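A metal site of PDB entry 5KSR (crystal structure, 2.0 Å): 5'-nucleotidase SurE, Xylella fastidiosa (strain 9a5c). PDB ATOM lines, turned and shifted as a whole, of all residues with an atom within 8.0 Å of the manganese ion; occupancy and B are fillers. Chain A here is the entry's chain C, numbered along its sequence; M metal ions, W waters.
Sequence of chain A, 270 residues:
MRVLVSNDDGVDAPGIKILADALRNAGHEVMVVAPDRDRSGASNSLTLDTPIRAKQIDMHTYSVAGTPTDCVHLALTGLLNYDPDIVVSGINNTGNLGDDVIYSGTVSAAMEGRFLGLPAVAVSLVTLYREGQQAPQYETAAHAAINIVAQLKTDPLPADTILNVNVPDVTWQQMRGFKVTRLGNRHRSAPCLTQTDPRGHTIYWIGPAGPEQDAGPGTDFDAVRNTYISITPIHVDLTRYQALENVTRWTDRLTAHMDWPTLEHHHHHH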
ATOM      1  N   ASN A   7      20.326  23.030  26.142  1.00  0.00           N
ATOM      2  CA  ASN A   7      21.362  23.759  26.954  1.00  0.00           C
ATOM      3  C   ASN A   7      21.528  25.265  26.566  1.00  0.00           C
ATOM      4  O   ASN A   7      20.782  25.750  25.718  1.00  0.00           O
ATOM      5  CB  ASN A   7      22.751  23.034  26.985  1.00  0.00           C
ATOM      6  CG  ASN A   7      23.598  23.230  25.695  1.00  0.00           C
ATOM      7  OD1 ASN A   7      23.193  23.885  24.723  1.00  0.00           O
ATOM      8  ND2 ASN A   7      24.810  22.682  25.704  1.00  0.00           N
ATOM      9  N   ASP A   8      22.483  25.998  27.174  1.00  0.00           N
ATOM     10  CA  ASP A   8      22.853  27.324  26.629  1.00  0.00           C
ATOM     11  C   ASP A   8      24.274  27.493  26.015  1.00  0.00           C
ATOM     12  O   ASP A   8      24.559  28.541  25.416  1.00  0.00           O
ATOM     13  CB  ASP A   8      22.481  28.511  27.570  1.00  0.00           C
ATOM     14  CG  ASP A   8      23.644  28.966  28.460  1.00  0.00           C
ATOM     15  OD1 ASP A   8      24.532  28.125  28.716  1.00  0.00           O
ATOM     16  OD2 ASP A   8      23.649  30.160  28.925  1.00  0.00           O
ATOM     17  N   ASP A   9      25.144  26.488  26.156  1.00  0.00           N
ATOM     18  CA  ASP A   9      26.501  26.535  25.589  1.00  0.00           C
ATOM     19  C   ASP A   9      26.604  26.153  24.100  1.00  0.00           C
ATOM     20  O   ASP A   9      27.646  26.387  23.471  1.00  0.00           O
ATOM     21  CB  ASP A   9      27.458  25.602  26.332  1.00  0.00           C
ATOM     22  CG  ASP A   9      27.656  25.974  27.772  1.00  0.00           C
ATOM     23  OD1 ASP A   9      27.716  27.190  28.096  1.00  0.00           O
ATOM     24  OD2 ASP A   9      27.791  25.022  28.593  1.00  0.00           O
ATOM     25  N   GLY A  10      25.570  25.523  23.560  1.00  0.00           N
ATOM     26  CA  GLY A  10      25.591  25.115  22.155  1.00  0.00           C
ATOM     27  C   GLY A  10      25.572  23.622  21.881  1.00  0.00           C
ATOM     28  O   GLY A  10      25.989  22.826  22.719  1.00  0.00           O
ATOM     29  N   ASP A  38      27.372  29.441  21.359  1.00  0.00           N
ATOM     30  CA  ASP A  38      27.255  29.868  22.782  1.00  0.00           C
ATOM     31  C   ASP A  38      26.479  31.180  22.946  1.00  0.00           C
ATOM     32  O   ASP A  38      26.830  32.207  22.358  1.00  0.00           O
ATOM     33  CB  ASP A  38      28.664  29.996  23.436  1.00  0.00           C
ATOM     34  CG  ASP A  38      28.633  30.067  24.992  1.00  0.00           C
ATOM     35  OD1 ASP A  38      27.670  30.583  25.594  1.00  0.00           O
ATOM     36  OD2 ASP A  38      29.622  29.623  25.627  1.00  0.00           O
ATOM     37  N   ARG A  39      25.445  31.139  23.778  1.00  0.00           N
ATOM     38  CA  ARG A  39      24.516  32.261  23.962  1.00  0.00           C
ATOM     39  C   ARG A  39      24.779  33.073  25.245  1.00  0.00           C
ATOM     40  O   ARG A  39      24.136  34.094  25.485  1.00  0.00           O
ATOM     41  CB  ARG A  39      23.063  31.744  23.939  1.00  0.00           C
ATOM     42  CG  ARG A  39      22.507  31.439  22.534  1.00  0.00           C
ATOM     43  CD  ARG A  39      21.731  32.647  21.977  1.00  0.00           C
ATOM     44  NE  ARG A  39      21.817  32.743  20.514  1.00  0.00           N
ATOM     45  CZ  ARG A  39      21.112  33.591  19.772  1.00  0.00           C
ATOM     46  NH1 ARG A  39      20.257  34.431  20.353  1.00  0.00           N
ATOM     47  NH2 ARG A  39      21.272  33.592  18.454  1.00  0.00           N
ATOM     48  N   SER A  40      25.721  32.605  26.056  1.00  0.00           N
ATOM     49  CA  SER A  40      26.107  33.295  27.289  1.00  0.00           C
ATOM     50  C   SER A  40      26.419  34.764  27.008  1.00  0.00           C
ATOM     51  O   SER A  40      27.425  35.082  26.380  1.00  0.00           O
ATOM     52  CB  SER A  40      27.316  32.616  27.932  1.00  0.00           C
ATOM     53  OG  SER A  40      27.095  31.215  28.154  1.00  0.00           O
ATOM     54  N   GLY A  41      25.545  35.665  27.453  1.00  0.00           N
ATOM     55  CA  GLY A  41      25.747  37.083  27.205  1.00  0.00           C
ATOM     56  C   GLY A  41      24.586  37.774  26.498  1.00  0.00           C
ATOM     57  O   GLY A  41      24.571  39.010  26.385  1.00  0.00           O
ATOM     58  N   ILE A  91      24.663  19.523  30.528  1.00  0.00           N
ATOM     59  CA  ILE A  91      25.313  19.937  31.793  1.00  0.00           C
ATOM     60  C   ILE A  91      26.162  21.223  31.541  1.00  0.00           C
ATOM     61  O   ILE A  91      27.088  21.183  30.731  1.00  0.00           O
ATOM     62  CB  ILE A  91      26.305  18.816  32.319  1.00  0.00           C
ATOM     63  CG1 ILE A  91      25.566  17.491  32.586  1.00  0.00           C
ATOM     64  CG2 ILE A  91      27.042  19.279  33.601  1.00  0.00           C
ATOM     65  CD1 ILE A  91      26.474  16.223  32.523  1.00  0.00           C
ATOM     66  N   ASN A  92      25.827  22.355  32.205  1.00  0.00           N
ATOM     67  CA  ASN A  92      26.581  23.630  32.060  1.00  0.00           C
ATOM     68  C   ASN A  92      28.064  23.592  32.512  1.00  0.00           C
ATOM     69  O   ASN A  92      28.389  22.911  33.484  1.00  0.00           O
ATOM     70  CB  ASN A  92      25.838  24.800  32.786  1.00  0.00           C
ATOM     71  CG  ASN A  92      26.254  26.188  32.296  1.00  0.00           C
ATOM     72  OD1 ASN A  92      26.095  26.512  31.115  1.00  0.00           O
ATOM     73  ND2 ASN A  92      26.743  27.029  33.215  1.00  0.00           N
ATOM     74  N   ASN A  93      28.948  24.300  31.819  1.00  0.00           N
ATOM     75  CA  ASN A  93      30.387  24.220  32.125  1.00  0.00           C
ATOM     76  C   ASN A  93      30.868  25.074  33.316  1.00  0.00           C
ATOM     77  O   ASN A  93      32.055  25.033  33.659  1.00  0.00           O
ATOM     78  CB  ASN A  93      31.262  24.443  30.873  1.00  0.00           C
ATOM     79  CG  ASN A  93      30.982  25.758  30.169  1.00  0.00           C
ATOM     80  OD1 ASN A  93      30.741  26.788  30.793  1.00  0.00           O
ATOM     81  ND2 ASN A  93      31.018  25.729  28.836  1.00  0.00           N
ATOM     82  N   THR A  94      29.953  25.824  33.946  1.00  0.00           N
ATOM     83  CA  THR A  94      30.230  26.526  35.225  1.00  0.00           C
ATOM     84  C   THR A  94      28.998  26.469  36.181  1.00  0.00           C
ATOM     85  O   THR A  94      27.893  26.112  35.747  1.00  0.00           O
ATOM     86  CB  THR A  94      30.541  28.038  35.034  1.00  0.00           C
ATOM     87  OG1 THR A  94      29.456  28.659  34.340  1.00  0.00           O
ATOM     88  CG2 THR A  94      31.822  28.254  34.235  1.00  0.00           C
ATOM     89  N   GLY A  95      29.183  26.844  37.450  1.00  0.00           N
ATOM     90  CA  GLY A  95      28.072  26.848  38.417  1.00  0.00           C
ATOM     91  C   GLY A  95      26.971  27.900  38.206  1.00  0.00           C
ATOM     92  O   GLY A  95      27.198  28.925  37.542  1.00  0.00           O
ATOM     93  N   ASN A  96      25.775  27.642  38.765  1.00  0.00           N
ATOM     94  CA  ASN A  96      24.647  28.610  38.767  1.00  0.00           C
ATOM     95  C   ASN A  96      24.047  28.737  40.197  1.00  0.00           C
ATOM     96  O   ASN A  96      23.109  28.005  40.541  1.00  0.00           O
ATOM     97  CB  ASN A  96      23.559  28.182  37.743  1.00  0.00           C
ATOM     98  CG  ASN A  96      23.963  28.418  36.267  1.00  0.00           C
ATOM     99  OD1 ASN A  96      24.131  27.456  35.473  1.00  0.00           O
ATOM    100  ND2 ASN A  96      24.075  29.683  35.884  1.00  0.00           N
ATOM    101  N   SER A 104      19.976  33.198  34.635  1.00  0.00           N
ATOM    102  CA  SER A 104      20.691  32.063  33.999  1.00  0.00           C
ATOM    103  C   SER A 104      20.023  31.506  32.713  1.00  0.00           C
ATOM    104  O   SER A 104      18.861  31.144  32.756  1.00  0.00           O
ATOM    105  CB  SER A 104      20.830  30.912  35.013  1.00  0.00           C
ATOM    106  OG  SER A 104      21.130  29.658  34.380  1.00  0.00           O
ATOM    107  N   GLY A 105      20.762  31.392  31.608  1.00  0.00           N
ATOM    108  CA  GLY A 105      20.221  30.810  30.374  1.00  0.00           C
ATOM    109  C   GLY A 105      19.879  29.325  30.505  1.00  0.00           C
ATOM    110  O   GLY A 105      18.886  28.863  29.917  1.00  0.00           O
ATOM    111  N   THR A 106      20.686  28.573  31.269  1.00  0.00           N
ATOM    112  CA  THR A 106      20.435  27.146  31.539  1.00  0.00           C
ATOM    113  C   THR A 106      19.083  26.946  32.262  1.00  0.00           C
ATOM    114  O   THR A 106      18.244  26.103  31.861  1.00  0.00           O
ATOM    115  CB  THR A 106      21.576  26.487  32.384  1.00  0.00           C
ATOM    116  OG1 THR A 106      22.859  26.644  31.750  1.00  0.00           O
ATOM    117  CG2 THR A 106      21.289  24.969  32.596  1.00  0.00           C
ATOM    118  N   SER A 124      24.197  21.717  36.543  1.00  0.00           N
ATOM    119  CA  SER A 124      25.465  22.483  36.325  1.00  0.00           C
ATOM    120  C   SER A 124      26.704  21.866  37.080  1.00  0.00           C
ATOM    121  O   SER A 124      26.549  21.347  38.197  1.00  0.00           O
ATOM    122  CB  SER A 124      25.302  23.960  36.778  1.00  0.00           C
ATOM    123  OG  SER A 124      24.125  24.628  36.247  1.00  0.00           O
HETATM  124 MN    MN M   1      26.609  28.535  29.833  1.00  0.00          MN
HETATM  125  O   HOH W   1      28.540  28.948  31.159  1.00  0.00           O
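Water W1 lies within hydrogen-bond range of the side-chain amide oxygen of Asn 93 (3.1 Å), the side-chain hydroxyl of Thr 94 (3.3 Å) and the side-chain amide nitrogen of Asn 92 (3.3 Å).
Ser 40 touches the manganese ion.
Of the 18 residues printed, 4 come within 4 Å of the manganese ion.
The manganese ion is bound by water W1 (2.4 Å), the side-chain carboxylate of Asp 8 (2.4 Å), the side-chain amide oxygen of Asn 92 (2.4 Å) and the side-chain carboxylate of Asp 9 (2.5 Å).
The manganese ion has four donor atoms within binding distance.
The backbone NH (N) of Arg 39 lies within hydrogen-bond range of the backbone carbonyl oxygen (O) of Asp 8, 3.2 Å away.
OD1 of Asn 92 sits close to OG1 of Thr 106 (3.3 Å).
The side-chain amide nitrogen (ND2) of Asn 92 lies within hydrogen-bond range of the backbone carbonyl oxygen (O) of Thr 94 (2.9 Å).
The side-chain amide nitrogen (ND2) of Asn 92 lies within hydrogen-bond range of the side-chain amide oxygen (OD1) of Asn 96, at 3.5 Å.
The side-chain amide nitrogen (ND2) of Asn 93 lies within hydrogen-bond range of the side-chain carboxylate (OD2) of Asp 9 (3.3 Å).
OG of Ser 40 lies within hydrogen-bond range of OD1 of Asp 38.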
